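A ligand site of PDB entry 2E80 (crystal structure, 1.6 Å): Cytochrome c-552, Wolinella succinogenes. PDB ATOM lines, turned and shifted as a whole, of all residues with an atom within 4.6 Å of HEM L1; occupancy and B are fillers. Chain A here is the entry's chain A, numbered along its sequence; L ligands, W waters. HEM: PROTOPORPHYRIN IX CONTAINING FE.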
ATOM      1  N   TYR A  74     -31.113 -11.593   0.130  1.00  0.00           N
ATOM      2  CA  TYR A  74     -29.876 -10.860   0.408  1.00  0.00           C
ATOM      3  C   TYR A  74     -29.117 -10.719  -0.901  1.00  0.00           C
ATOM      4  O   TYR A  74     -28.642 -11.708  -1.462  1.00  0.00           O
ATOM      5  CB  TYR A  74     -29.017 -11.611   1.431  1.00  0.00           C
ATOM      6  CG  TYR A  74     -27.633 -11.029   1.607  1.00  0.00           C
ATOM      7  CD1 TYR A  74     -27.453  -9.702   2.020  1.00  0.00           C
ATOM      8  CD2 TYR A  74     -26.495 -11.783   1.316  1.00  0.00           C
ATOM      9  CE1 TYR A  74     -26.171  -9.150   2.138  1.00  0.00           C
ATOM     10  CE2 TYR A  74     -25.219 -11.242   1.429  1.00  0.00           C
ATOM     11  CZ  TYR A  74     -25.059  -9.930   1.842  1.00  0.00           C
ATOM     12  OH  TYR A  74     -23.788  -9.396   1.937  1.00  0.00           O
ATOM     13  N   ASN A  75     -29.018  -9.487  -1.388  1.00  0.00           N
ATOM     14  CA  ASN A  75     -28.322  -9.220  -2.644  1.00  0.00           C
ATOM     15  C   ASN A  75     -27.124  -8.306  -2.427  1.00  0.00           C
ATOM     16  O   ASN A  75     -27.016  -7.663  -1.384  1.00  0.00           O
ATOM     17  CB  ASN A  75     -29.279  -8.556  -3.641  1.00  0.00           C
ATOM     18  CG  ASN A  75     -30.590  -9.295  -3.752  1.00  0.00           C
ATOM     19  OD1 ASN A  75     -30.614 -10.510  -3.932  1.00  0.00           O
ATOM     20  ND2 ASN A  75     -31.696  -8.569  -3.637  1.00  0.00           N
ATOM     21  N   ALA A  76     -26.235  -8.257  -3.404  1.00  0.00           N
ATOM     22  CA  ALA A  76     -25.043  -7.413  -3.314  1.00  0.00           C
ATOM     23  C   ALA A  76     -25.475  -5.954  -3.456  1.00  0.00           C
ATOM     24  O   ALA A  76     -26.554  -5.667  -3.957  1.00  0.00           O
ATOM     25  CB  ALA A  76     -24.061  -7.769  -4.421  1.00  0.00           C
ATOM     26  N   PRO A  77     -24.621  -5.015  -3.013  1.00  0.00           N
ATOM     27  CA  PRO A  77     -24.964  -3.594  -3.102  1.00  0.00           C
ATOM     28  C   PRO A  77     -24.903  -3.088  -4.536  1.00  0.00           C
ATOM     29  O   PRO A  77     -24.034  -3.503  -5.302  1.00  0.00           O
ATOM     30  CB  PRO A  77     -23.895  -2.905  -2.252  1.00  0.00           C
ATOM     31  CG  PRO A  77     -23.278  -4.014  -1.429  1.00  0.00           C
ATOM     32  CD  PRO A  77     -23.319  -5.194  -2.352  1.00  0.00           C
ATOM     33  N   ASP A  86     -34.709  -0.722  -3.014  1.00  0.00           N
ATOM     34  CA  ASP A  86     -34.277  -2.064  -2.627  1.00  0.00           C
ATOM     35  C   ASP A  86     -34.722  -2.370  -1.190  1.00  0.00           C
ATOM     36  O   ASP A  86     -35.021  -3.515  -0.861  1.00  0.00           O
ATOM     37  CB  ASP A  86     -32.765  -2.207  -2.789  1.00  0.00           C
ATOM     38  CG  ASP A  86     -32.355  -2.315  -4.249  1.00  0.00           C
ATOM     39  OD1 ASP A  86     -33.225  -2.619  -5.082  1.00  0.00           O
ATOM     40  OD2 ASP A  86     -31.164  -2.100  -4.570  1.00  0.00           O
ATOM     41  N   ASN A  87     -34.778  -1.336  -0.364  1.00  0.00           N
ATOM     42  CA  ASN A  87     -35.220  -1.450   1.028  1.00  0.00           C
ATOM     43  C   ASN A  87     -36.694  -1.906   0.978  1.00  0.00           C
ATOM     44  O   ASN A  87     -37.120  -2.747   1.769  1.00  0.00           O
ATOM     45  CB  ASN A  87     -35.080  -0.086   1.704  1.00  0.00           C
ATOM     46  CG  ASN A  87     -35.373  -0.111   3.196  1.00  0.00           C
ATOM     47  OD1 ASN A  87     -36.264   0.595   3.671  1.00  0.00           O
ATOM     48  ND2 ASN A  87     -34.624  -0.921   3.943  1.00  0.00           N
ATOM     49  N   THR A  90     -36.800  -5.796  -0.906  1.00  0.00           N
ATOM     50  CA  THR A  90     -36.289  -6.988  -0.231  1.00  0.00           C
ATOM     51  C   THR A  90     -37.345  -7.753   0.546  1.00  0.00           C
ATOM     52  O   THR A  90     -38.198  -7.174   1.218  1.00  0.00           O
ATOM     53  CB  THR A  90     -35.125  -6.648   0.731  1.00  0.00           C
ATOM     54  OG1 THR A  90     -34.638  -7.863   1.311  1.00  0.00           O
ATOM     55  CG2 THR A  90     -35.592  -5.714   1.858  1.00  0.00           C
ATOM     56  N   ARG A  92     -36.932  -9.183   3.079  1.00  0.00           N
ATOM     57  CA  ARG A  92     -36.689  -8.983   4.498  1.00  0.00           C
ATOM     58  C   ARG A  92     -37.695  -8.041   5.157  1.00  0.00           C
ATOM     59  O   ARG A  92     -38.036  -8.235   6.327  1.00  0.00           O
ATOM     60  CB  ARG A  92     -35.268  -8.480   4.746  1.00  0.00           C
ATOM     61  CG  ARG A  92     -34.184  -9.403   4.177  1.00  0.00           C
ATOM     62  CD  ARG A  92     -32.874  -9.284   4.942  1.00  0.00           C
ATOM     63  NE  ARG A  92     -32.234  -7.970   4.837  1.00  0.00           N
ATOM     64  CZ  ARG A  92     -31.483  -7.564   3.823  1.00  0.00           C
ATOM     65  NH1 ARG A  92     -31.262  -8.359   2.778  1.00  0.00           N
ATOM     66  NH2 ARG A  92     -30.919  -6.366   3.858  1.00  0.00           N
ATOM     67  N   THR A  93     -38.179  -7.046   4.422  1.00  0.00           N
ATOM     68  CA  THR A  93     -39.158  -6.119   5.001  1.00  0.00           C
ATOM     69  C   THR A  93     -40.593  -6.649   4.933  1.00  0.00           C
ATOM     70  O   THR A  93     -41.523  -5.993   5.392  1.00  0.00           O
ATOM     71  CB  THR A  93     -39.066  -4.727   4.341  1.00  0.00           C
ATOM     72  OG1 THR A  93     -39.032  -4.868   2.907  1.00  0.00           O
ATOM     73  CG2 THR A  93     -37.812  -3.988   4.821  1.00  0.00           C
ATOM     74  N   LEU A 104     -40.302  -5.848  10.197  1.00  0.00           N
ATOM     75  CA  LEU A 104     -39.248  -4.938  10.645  1.00  0.00           C
ATOM     76  C   LEU A 104     -39.674  -3.563  11.180  1.00  0.00           C
ATOM     77  O   LEU A 104     -40.760  -3.072  10.875  1.00  0.00           O
ATOM     78  CB  LEU A 104     -38.202  -4.795   9.536  1.00  0.00           C
ATOM     79  CG  LEU A 104     -37.661  -6.163   9.074  1.00  0.00           C
ATOM     80  CD1 LEU A 104     -36.551  -5.978   8.040  1.00  0.00           C
ATOM     81  CD2 LEU A 104     -37.137  -6.926  10.278  1.00  0.00           C
ATOM     82  N   ALA A 107     -36.388   1.689  12.071  1.00  0.00           N
ATOM     83  CA  ALA A 107     -34.955   1.895  11.911  1.00  0.00           C
ATOM     84  C   ALA A 107     -34.404   1.419  10.569  1.00  0.00           C
ATOM     85  O   ALA A 107     -33.325   1.833  10.158  1.00  0.00           O
ATOM     86  CB  ALA A 107     -34.197   1.225  13.057  1.00  0.00           C
ATOM     87  N   CYS A 108     -35.153   0.570   9.865  1.00  0.00           N
ATOM     88  CA  CYS A 108     -34.660   0.076   8.579  1.00  0.00           C
ATOM     89  C   CYS A 108     -34.593   1.132   7.471  1.00  0.00           C
ATOM     90  O   CYS A 108     -34.026   0.859   6.416  1.00  0.00           O
ATOM     91  CB  CYS A 108     -35.485  -1.129   8.109  1.00  0.00           C
ATOM     92  SG  CYS A 108     -35.125  -2.650   9.029  1.00  0.00           S
ATOM     93  N   THR A 110     -33.356   4.225   8.092  1.00  0.00           N
ATOM     94  CA  THR A 110     -32.236   5.046   8.517  1.00  0.00           C
ATOM     95  C   THR A 110     -31.105   5.369   7.540  1.00  0.00           C
ATOM     96  O   THR A 110     -30.727   6.533   7.400  1.00  0.00           O
ATOM     97  CB  THR A 110     -31.622   4.479   9.814  1.00  0.00           C
ATOM     98  OG1 THR A 110     -32.671   4.217  10.747  1.00  0.00           O
ATOM     99  CG2 THR A 110     -30.646   5.481  10.430  1.00  0.00           C
ATOM    100  N   CYS A 111     -30.577   4.358   6.860  1.00  0.00           N
ATOM    101  CA  CYS A 111     -29.474   4.566   5.942  1.00  0.00           C
ATOM    102  C   CYS A 111     -29.864   4.446   4.473  1.00  0.00           C
ATOM    103  O   CYS A 111     -29.065   4.020   3.644  1.00  0.00           O
ATOM    104  CB  CYS A 111     -28.365   3.567   6.260  1.00  0.00           C
ATOM    105  SG  CYS A 111     -27.875   3.528   8.017  1.00  0.00           S
ATOM    106  N   LYS A 112     -31.091   4.840   4.156  1.00  0.00           N
ATOM    107  CA  LYS A 112     -31.586   4.728   2.804  1.00  0.00           C
ATOM    108  C   LYS A 112     -32.153   6.010   2.215  1.00  0.00           C
ATOM    109  O   LYS A 112     -32.431   6.065   1.015  1.00  0.00           O
ATOM    110  CB  LYS A 112     -32.707   3.678   2.776  1.00  0.00           C
ATOM    111  CG  LYS A 112     -32.340   2.320   3.342  1.00  0.00           C
ATOM    112  CD  LYS A 112     -31.429   1.569   2.393  1.00  0.00           C
ATOM    113  CE  LYS A 112     -31.141   0.165   2.888  1.00  0.00           C
ATOM    114  NZ  LYS A 112     -30.262   0.136   4.085  1.00  0.00           N
ATOM    115  N   TYR A 163     -26.180   8.728  16.054  1.00  0.00           N
ATOM    116  CA  TYR A 163     -25.519   7.497  16.465  1.00  0.00           C
ATOM    117  C   TYR A 163     -24.059   7.362  16.019  1.00  0.00           C
ATOM    118  O   TYR A 163     -23.292   6.615  16.639  1.00  0.00           O
ATOM    119  CB  TYR A 163     -26.329   6.267  16.032  1.00  0.00           C
ATOM    120  CG  TYR A 163     -26.526   6.108  14.541  1.00  0.00           C
ATOM    121  CD1 TYR A 163     -25.468   5.723  13.719  1.00  0.00           C
ATOM    122  CD2 TYR A 163     -27.771   6.334  13.957  1.00  0.00           C
ATOM    123  CE1 TYR A 163     -25.641   5.560  12.343  1.00  0.00           C
ATOM    124  CE2 TYR A 163     -27.962   6.181  12.583  1.00  0.00           C
ATOM    125  CZ  TYR A 163     -26.887   5.801  11.787  1.00  0.00           C
ATOM    126  OH  TYR A 163     -27.064   5.649  10.430  1.00  0.00           O
ATOM    127  N   GLN A 191     -21.741   7.052   8.110  1.00  0.00           N
ATOM    128  CA  GLN A 191     -23.058   7.231   8.707  1.00  0.00           C
ATOM    129  C   GLN A 191     -23.859   5.956   8.440  1.00  0.00           C
ATOM    130  O   GLN A 191     -24.724   5.562   9.220  1.00  0.00           O
ATOM    131  CB  GLN A 191     -23.815   8.378   8.056  1.00  0.00           C
ATOM    132  CG  GLN A 191     -23.181   9.738   8.168  1.00  0.00           C
ATOM    133  CD  GLN A 191     -24.034  10.789   7.501  1.00  0.00           C
ATOM    134  OE1 GLN A 191     -25.043  11.244   8.065  1.00  0.00           O
ATOM    135  NE2 GLN A 191     -23.663  11.163   6.284  1.00  0.00           N
ATOM    136  N   CYS A 192     -23.557   5.316   7.317  1.00  0.00           N
ATOM    137  CA  CYS A 192     -24.282   4.115   6.903  1.00  0.00           C
ATOM    138  C   CYS A 192     -23.459   2.859   6.715  1.00  0.00           C
ATOM    139  O   CYS A 192     -23.906   1.756   7.041  1.00  0.00           O
ATOM    140  CB  CYS A 192     -25.024   4.392   5.602  1.00  0.00           C
ATOM    141  SG  CYS A 192     -25.971   5.915   5.604  1.00  0.00           S
ATOM    142  N   HIS A 193     -22.262   3.008   6.162  1.00  0.00           N
ATOM    143  CA  HIS A 193     -21.389   1.872   5.873  1.00  0.00           C
ATOM    144  C   HIS A 193     -20.608   1.363   7.077  1.00  0.00           C
ATOM    145  O   HIS A 193     -19.377   1.358   7.084  1.00  0.00           O
ATOM    146  CB  HIS A 193     -20.441   2.248   4.734  1.00  0.00           C
ATOM    147  CG  HIS A 193     -21.107   2.265   3.389  1.00  0.00           C
ATOM    148  ND1 HIS A 193     -21.210   1.162   2.568  1.00  0.00           N
ATOM    149  CD2 HIS A 193     -21.756   3.270   2.743  1.00  0.00           C
ATOM    150  CE1 HIS A 193     -21.910   1.516   1.469  1.00  0.00           C
ATOM    151  NE2 HIS A 193     -22.253   2.792   1.529  1.00  0.00           N
ATOM    152  N   VAL A 194     -21.350   0.912   8.082  1.00  0.00           N
ATOM    153  CA  VAL A 194     -20.779   0.385   9.323  1.00  0.00           C
ATOM    154  C   VAL A 194     -21.676  -0.723   9.885  1.00  0.00           C
ATOM    155  O   VAL A 194     -22.816  -0.884   9.468  1.00  0.00           O
ATOM    156  CB  VAL A 194     -20.674   1.499  10.392  1.00  0.00           C
ATOM    157  CG1 VAL A 194     -19.636   2.535   9.988  1.00  0.00           C
ATOM    158  CG2 VAL A 194     -22.030   2.160  10.583  1.00  0.00           C
ATOM    159  N   TYR A 196     -23.899  -2.434  12.854  1.00  0.00           N
ATOM    160  CA  TYR A 196     -24.788  -1.874  13.852  1.00  0.00           C
ATOM    161  C   TYR A 196     -25.700  -2.951  14.440  1.00  0.00           C
ATOM    162  O   TYR A 196     -25.707  -4.088  13.987  1.00  0.00           O
ATOM    163  CB  TYR A 196     -25.691  -0.813  13.208  1.00  0.00           C
ATOM    164  CG  TYR A 196     -26.773  -1.433  12.339  1.00  0.00           C
ATOM    165  CD1 TYR A 196     -26.504  -1.876  11.047  1.00  0.00           C
ATOM    166  CD2 TYR A 196     -28.039  -1.691  12.873  1.00  0.00           C
ATOM    167  CE1 TYR A 196     -27.478  -2.559  10.299  1.00  0.00           C
ATOM    168  CE2 TYR A 196     -29.000  -2.372  12.142  1.00  0.00           C
ATOM    169  CZ  TYR A 196     -28.721  -2.801  10.865  1.00  0.00           C
ATOM    170  OH  TYR A 196     -29.684  -3.493  10.161  1.00  0.00           O
ATOM    171  N   PHE A 198     -29.789  -3.098  16.673  1.00  0.00           N
ATOM    172  CA  PHE A 198     -30.918  -2.315  17.183  1.00  0.00           C
ATOM    173  C   PHE A 198     -31.008  -2.498  18.690  1.00  0.00           C
ATOM    174  O   PHE A 198     -31.163  -3.620  19.177  1.00  0.00           O
ATOM    175  CB  PHE A 198     -32.239  -2.774  16.549  1.00  0.00           C
ATOM    176  CG  PHE A 198     -32.363  -2.488  15.081  1.00  0.00           C
ATOM    177  CD1 PHE A 198     -31.694  -1.401  14.507  1.00  0.00           C
ATOM    178  CD2 PHE A 198     -33.172  -3.274  14.275  1.00  0.00           C
ATOM    179  CE1 PHE A 198     -31.851  -1.119  13.149  1.00  0.00           C
ATOM    180  CE2 PHE A 198     -33.333  -3.000  12.921  1.00  0.00           C
ATOM    181  CZ  PHE A 198     -32.674  -1.914  12.361  1.00  0.00           C
ATOM    182  N   VAL A 216     -30.647   2.508  16.322  1.00  0.00           N
ATOM    183  CA  VAL A 216     -29.433   2.084  15.642  1.00  0.00           C
ATOM    184  C   VAL A 216     -28.261   2.408  16.553  1.00  0.00           C
ATOM    185  O   VAL A 216     -28.070   3.565  16.945  1.00  0.00           O
ATOM    186  CB  VAL A 216     -29.250   2.824  14.310  1.00  0.00           C
ATOM    187  CG1 VAL A 216     -27.892   2.488  13.700  1.00  0.00           C
ATOM    188  CG2 VAL A 216     -30.358   2.439  13.357  1.00  0.00           C
ATOM    189  N   HIS A 255     -22.291  -5.069   6.771  1.00  0.00           N
ATOM    190  CA  HIS A 255     -21.369  -4.189   6.082  1.00  0.00           C
ATOM    191  C   HIS A 255     -20.511  -3.281   6.963  1.00  0.00           C
ATOM    192  O   HIS A 255     -20.761  -2.075   7.064  1.00  0.00           O
ATOM    193  CB  HIS A 255     -22.163  -3.323   5.110  1.00  0.00           C
ATOM    194  CG  HIS A 255     -23.432  -2.785   5.701  1.00  0.00           C
ATOM    195  ND1 HIS A 255     -23.434  -1.923   6.769  1.00  0.00           N
ATOM    196  CD2 HIS A 255     -24.727  -3.059   5.426  1.00  0.00           C
ATOM    197  CE1 HIS A 255     -24.687  -1.674   7.125  1.00  0.00           C
ATOM    198  NE2 HIS A 255     -25.486  -2.354   6.323  1.00  0.00           N
ATOM    199  N   ASP A 257     -17.981  -1.739   6.554  1.00  0.00           N
ATOM    200  CA  ASP A 257     -17.089  -1.136   5.585  1.00  0.00           C
ATOM    201  C   ASP A 257     -16.052  -0.189   6.190  1.00  0.00           C
ATOM    202  O   ASP A 257     -14.859  -0.338   5.939  1.00  0.00           O
ATOM    203  CB  ASP A 257     -17.898  -0.408   4.511  1.00  0.00           C
ATOM    204  CG  ASP A 257     -18.969  -1.285   3.891  1.00  0.00           C
ATOM    205  OD1 ASP A 257     -18.642  -2.410   3.433  1.00  0.00           O
ATOM    206  OD2 ASP A 257     -20.145  -0.856   3.844  1.00  0.00           O
ATOM    207  N   ALA A 376     -19.220  -9.449   5.081  1.00  0.00           N
ATOM    208  CA  ALA A 376     -20.364  -8.531   5.010  1.00  0.00           C
ATOM    209  C   ALA A 376     -20.035  -7.233   4.278  1.00  0.00           C
ATOM    210  O   ALA A 376     -20.898  -6.628   3.647  1.00  0.00           O
ATOM    211  CB  ALA A 376     -20.900  -8.238   6.410  1.00  0.00           C
ATOM    212  N   HIS A 378     -18.538  -5.915   1.276  1.00  0.00           N
ATOM    213  CA  HIS A 378     -18.140  -6.435  -0.027  1.00  0.00           C
ATOM    214  C   HIS A 378     -16.806  -5.948  -0.595  1.00  0.00           C
ATOM    215  O   HIS A 378     -16.224  -6.587  -1.473  1.00  0.00           O
ATOM    216  CB  HIS A 378     -19.250  -6.174  -1.037  1.00  0.00           C
ATOM    217  CG  HIS A 378     -20.491  -6.976  -0.785  1.00  0.00           C
ATOM    218  ND1 HIS A 378     -20.648  -8.273  -1.237  1.00  0.00           N
ATOM    219  CD2 HIS A 378     -21.601  -6.689  -0.067  1.00  0.00           C
ATOM    220  CE1 HIS A 378     -21.810  -8.740  -0.816  1.00  0.00           C
ATOM    221  NE2 HIS A 378     -22.401  -7.795  -0.106  1.00  0.00           N
HETATM  222  CHA HEM L   1     -27.928  -2.349   1.898  1.00  0.00           C
HETATM  223  CHB HEM L   1     -32.205  -3.342   3.841  1.00  0.00           C
HETATM  224  CHC HEM L   1     -30.788  -1.314   7.984  1.00  0.00           C
HETATM  225  CHD HEM L   1     -26.941   0.410   5.655  1.00  0.00           C
HETATM  226  C1A HEM L   1     -29.236  -2.771   2.051  1.00  0.00           C
HETATM  227  C2A HEM L   1     -29.984  -3.502   1.043  1.00  0.00           C
HETATM  228  C3A HEM L   1     -31.192  -3.781   1.589  1.00  0.00           C
HETATM  229  C4A HEM L   1     -31.189  -3.215   2.921  1.00  0.00           C
HETATM  230  CMA HEM L   1     -32.299  -4.607   0.919  1.00  0.00           C
HETATM  231  CAA HEM L   1     -29.457  -3.928  -0.342  1.00  0.00           C
HETATM  232  CBA HEM L   1     -28.619  -5.197  -0.267  1.00  0.00           C
HETATM  233  CGA HEM L   1     -29.411  -6.391   0.216  1.00  0.00           C
HETATM  234  O1A HEM L   1     -30.247  -6.908  -0.554  1.00  0.00           O
HETATM  235  O2A HEM L   1     -29.213  -6.811   1.378  1.00  0.00           O
HETATM  236  C1B HEM L   1     -32.208  -2.892   5.149  1.00  0.00           C
HETATM  237  C2B HEM L   1     -33.203  -3.281   6.142  1.00  0.00           C
HETATM  238  C3B HEM L   1     -32.779  -2.765   7.343  1.00  0.00           C
HETATM  239  C4B HEM L   1     -31.538  -2.043   7.052  1.00  0.00           C
HETATM  240  CMB HEM L   1     -34.438  -4.148   5.887  1.00  0.00           C
HETATM  241  CAB HEM L   1     -33.368  -2.982   8.606  1.00  0.00           C
HETATM  242  CBB HEM L   1     -33.142  -4.189   9.327  1.00  0.00           C
HETATM  243  C1C HEM L   1     -29.597  -0.647   7.705  1.00  0.00           C
HETATM  244  C2C HEM L   1     -28.951   0.306   8.602  1.00  0.00           C
HETATM  245  C3C HEM L   1     -27.891   0.856   7.930  1.00  0.00           C
HETATM  246  C4C HEM L   1     -27.875   0.187   6.627  1.00  0.00           C
HETATM  247  CMC HEM L   1     -29.462   0.672  10.003  1.00  0.00           C
HETATM  248  CAC HEM L   1     -27.047   1.919   8.323  1.00  0.00           C
HETATM  249  CBC HEM L   1     -26.447   2.010   9.606  1.00  0.00           C
HETATM  250  C1D HEM L   1     -26.844  -0.236   4.452  1.00  0.00           C
HETATM  251  C2D HEM L   1     -25.671  -0.190   3.590  1.00  0.00           C
HETATM  252  C3D HEM L   1     -25.894  -1.095   2.616  1.00  0.00           C
HETATM  253  C4D HEM L   1     -27.215  -1.652   2.852  1.00  0.00           C
HETATM  254  CMD HEM L   1     -24.445   0.702   3.762  1.00  0.00           C
HETATM  255  CAD HEM L   1     -24.967  -1.382   1.425  1.00  0.00           C
HETATM  256  CBD HEM L   1     -23.740  -2.254   1.621  1.00  0.00           C
HETATM  257  CGD HEM L   1     -24.073  -3.723   1.743  1.00  0.00           C
HETATM  258  O1D HEM L   1     -25.237  -4.110   1.532  1.00  0.00           O
HETATM  259  O2D HEM L   1     -23.152  -4.512   2.046  1.00  0.00           O
HETATM  260  NA  HEM L   1     -29.982  -2.581   3.188  1.00  0.00           N
HETATM  261  NB  HEM L   1     -31.173  -2.180   5.715  1.00  0.00           N
HETATM  262  NC  HEM L   1     -28.951  -0.684   6.491  1.00  0.00           N
HETATM  263  ND  HEM L   1     -27.779  -1.154   4.004  1.00  0.00           N
HETATM  264 FE   HEM L   1     -29.484  -1.660   4.854  1.00  0.00          FE
HETATM  265  CHA HEM L   2     -24.182   1.211  -1.845  1.00  0.00           C
HETATM  266  CHB HEM L   2     -20.030   3.599  -1.251  1.00  0.00           C
HETATM  267  CHC HEM L   2     -22.242   6.802   1.498  1.00  0.00           C
HETATM  268  CHD HEM L   2     -25.897   3.745   1.854  1.00  0.00           C
HETATM  269  C1A HEM L   2     -22.920   1.743  -2.087  1.00  0.00           C
HETATM  270  C2A HEM L   2     -21.996   1.192  -3.032  1.00  0.00           C
HETATM  271  C3A HEM L   2     -20.799   1.819  -2.815  1.00  0.00           C
HETATM  272  C4A HEM L   2     -21.008   2.736  -1.727  1.00  0.00           C
HETATM  273  CMA HEM L   2     -19.504   1.621  -3.597  1.00  0.00           C
HETATM  274  CAA HEM L   2     -22.300   0.158  -4.124  1.00  0.00           C
HETATM  275  CBA HEM L   2     -22.131   0.811  -5.477  1.00  0.00           C
HETATM  276  CGA HEM L   2     -22.489  -0.116  -6.622  1.00  0.00           C
HETATM  277  O1A HEM L   2     -22.527  -1.340  -6.410  1.00  0.00           O
HETATM  278  O2A HEM L   2     -22.720   0.403  -7.732  1.00  0.00           O
HETATM  279  C1B HEM L   2     -20.244   4.680  -0.426  1.00  0.00           C
HETATM  280  C2B HEM L   2     -19.255   5.713  -0.111  1.00  0.00           C
HETATM  281  C3B HEM L   2     -19.904   6.678   0.609  1.00  0.00           C
HETATM  282  C4B HEM L   2     -21.269   6.190   0.747  1.00  0.00           C
HETATM  283  CMB HEM L   2     -17.784   5.720  -0.499  1.00  0.00           C
HETATM  284  CAB HEM L   2     -19.406   7.908   1.070  1.00  0.00           C
HETATM  285  CBB HEM L   2     -18.899   8.870   0.159  1.00  0.00           C
HETATM  286  C1C HEM L   2     -23.480   6.286   1.772  1.00  0.00           C
HETATM  287  C2C HEM L   2     -24.369   6.852   2.757  1.00  0.00           C
HETATM  288  C3C HEM L   2     -25.373   5.957   2.937  1.00  0.00           C
HETATM  289  C4C HEM L   2     -25.093   4.845   2.037  1.00  0.00           C
HETATM  290  CMC HEM L   2     -24.184   8.174   3.511  1.00  0.00           C
HETATM  291  CAC HEM L   2     -26.425   6.092   3.843  1.00  0.00           C
HETATM  292  CBC HEM L   2     -27.361   7.169   3.776  1.00  0.00           C
HETATM  293  C1D HEM L   2     -25.737   2.764   0.912  1.00  0.00           C
HETATM  294  C2D HEM L   2     -26.769   1.785   0.569  1.00  0.00           C
HETATM  295  C3D HEM L   2     -26.302   1.095  -0.477  1.00  0.00           C
HETATM  296  C4D HEM L   2     -25.001   1.637  -0.811  1.00  0.00           C
HETATM  297  CMD HEM L   2     -28.063   1.543   1.359  1.00  0.00           C
HETATM  298  CAD HEM L   2     -27.025  -0.062  -1.148  1.00  0.00           C
HETATM  299  CBD HEM L   2     -27.747   0.418  -2.405  1.00  0.00           C
HETATM  300  CGD HEM L   2     -28.564  -0.685  -3.055  1.00  0.00           C
HETATM  301  O1D HEM L   2     -28.048  -1.812  -3.163  1.00  0.00           O
HETATM  302  O2D HEM L   2     -29.719  -0.414  -3.462  1.00  0.00           O
HETATM  303  NA  HEM L   2     -22.317   2.729  -1.310  1.00  0.00           N
HETATM  304  NB  HEM L   2     -21.449   4.981   0.106  1.00  0.00           N
HETATM  305  NC  HEM L   2     -23.931   5.058   1.308  1.00  0.00           N
HETATM  306  ND  HEM L   2     -24.671   2.690   0.047  1.00  0.00           N
HETATM  307 FE   HEM L   2     -23.103   3.873   0.027  1.00  0.00          FE
HETATM  308  O   HOH W   1     -25.017  -6.693   0.233  1.00  0.00           O
HETATM  309  O   HOH W   2     -31.460   1.607   6.587  1.00  0.00           O
HETATM  310  O   HOH W   3     -30.550  -0.597  -0.435  1.00  0.00           O
HETATM  311  O   HOH W   4     -27.094  -5.802   2.890  1.00  0.00           O
HETATM  312  O   HOH W   5     -31.783  -6.368   7.052  1.00  0.00           O
HETATM  313  O   HOH W   6     -20.492  -3.757   1.571  1.00  0.00           O
HETATM  314  O   HOH W   7     -23.353  -6.953   2.890  1.00  0.00           O
HETATM  315  O   HOH W   8     -32.498  -8.466  -0.289  1.00  0.00           O
HETATM  316  O   HOH W   9     -31.349  -5.741  -2.713  1.00  0.00           O
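A carbon (CAC) of HEM L2 is bonded to the side-chain sulfur (SG) of Cys 192.
The side-chain amino group (NZ) of Lys 112 is bound to an iron atom (FE) of HEM L1, at 2.1 Å.
The side-chain sulfur (SG) of Cys 111 is bonded to a carbon (CAC) of HEM L1 (1.8 Å).
A ring nitrogen (NE2) of His 193 binds an iron atom (FE) of HEM L2, at 2.0 Å.
O2A of HEM L1 lies within salt-bridge range of NH1 of Arg 92, at 2.9 Å.
An oxygen (O1A) of HEM L1 sits at hydrogen-bond distance from the backbone NH (N) of Asn 75 (3.0 Å).
SG of Cys 108 is covalently linked to CAB of HEM L1 (1.8 Å).
An oxygen (O2D) of HEM L2 sits close to the side-chain carboxylate of Asp 86 (2.5 Å).
The side-chain amide nitrogen (ND2) of Asn 87 sits at hydrogen-bond distance from the backbone carbonyl oxygen (O) of Cys 108.
A ring nitrogen (ND1) of His 255 sits at hydrogen-bond distance from the backbone carbonyl oxygen of Val 194 (3.0 Å).
The backbone NH (N) of Arg 92 sits close to the side-chain hydroxyl (OG1) of Thr 90, 3.2 Å away.
The side-chain hydroxyl of Tyr 163 lies within hydrogen-bond range of the backbone carbonyl oxygen of Gln 191.
The side-chain hydroxyl of Tyr 163 sits at hydrogen-bond distance from the side-chain sulfur of Cys 111, 3.3 Å away.
OG1 of Thr 93 lies within hydrogen-bond range of O of Asn 87, 3.1 Å away.
O of Thr 90 sits at hydrogen-bond distance from OG1 of Thr 93 (3.0 Å).
A ring nitrogen (ND1) of His 193 lies within hydrogen-bond range of the side-chain carboxylate (OD2) of Asp 257, 2.6 Å away.
NE2 of His 255 sits close to ND of HEM L1, at 3.5 Å.
O2D of HEM L1 sits close to O of Ala 376, at 3.5 Å.
Merely in contact with HEM L1: Tyr 74 (3.4 Å), Pro 77 (3.3 Å), Asp 86 (3.4 Å), Asn 87 (3.3 Å), Thr 90 (3.5 Å), Thr 93 (3.5 Å), Leu 104 (3.5 Å), Tyr 163 (3.8 Å), Gln 191 (3.97 Å), Cys 192 (3.4 Å), His 193 (3.5 Å), Tyr 196 (3.3 Å), Phe 198 (3.8 Å), Val 216 (3.9 Å) and His 378 (3.4 Å).
Hydrophobic or aromatic side chains within 4 Å of HEM L1: Tyr 74, Pro 77, Leu 104, His 193, Tyr 196, Phe 198, Val 216, His 255 and His 378.
22 residues have an atom within 4 Å of HEM L1: Tyr 74, Asn 75, Pro 77, Asp 86, Asn 87, Thr 90, Arg 92, Thr 93, Leu 104, Cys 108, Cys 111, Lys 112, Tyr 163, Gln 191, Cys 192, His 193, Tyr 196, Phe 198, Val 216, His 255, Ala 376 and His 378.
Water W7 lies within hydrogen-bond range of O of Ala 376 (2.6 Å), O2D of HEM L1 (2.6 Å), OH of Tyr 74 (2.7 Å) and NE2 of His 378 (3.3 Å).
Water W9 bridges O1A of HEM L1 (2.7 Å) and ND2 of Asn 75 (3.0 Å).
Water W6 lies within hydrogen-bond range of O2D of HEM L1 (2.8 Å), N of His 378 (2.9 Å) and OD1 of Asp 257 (3.0 Å).
Water W1 lies within hydrogen-bond range of O of Asn 75 (2.7 Å), NE2 of His 378 (2.9 Å), O1D of HEM L1 (2.9 Å) and OH of Tyr 74 (3.4 Å).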
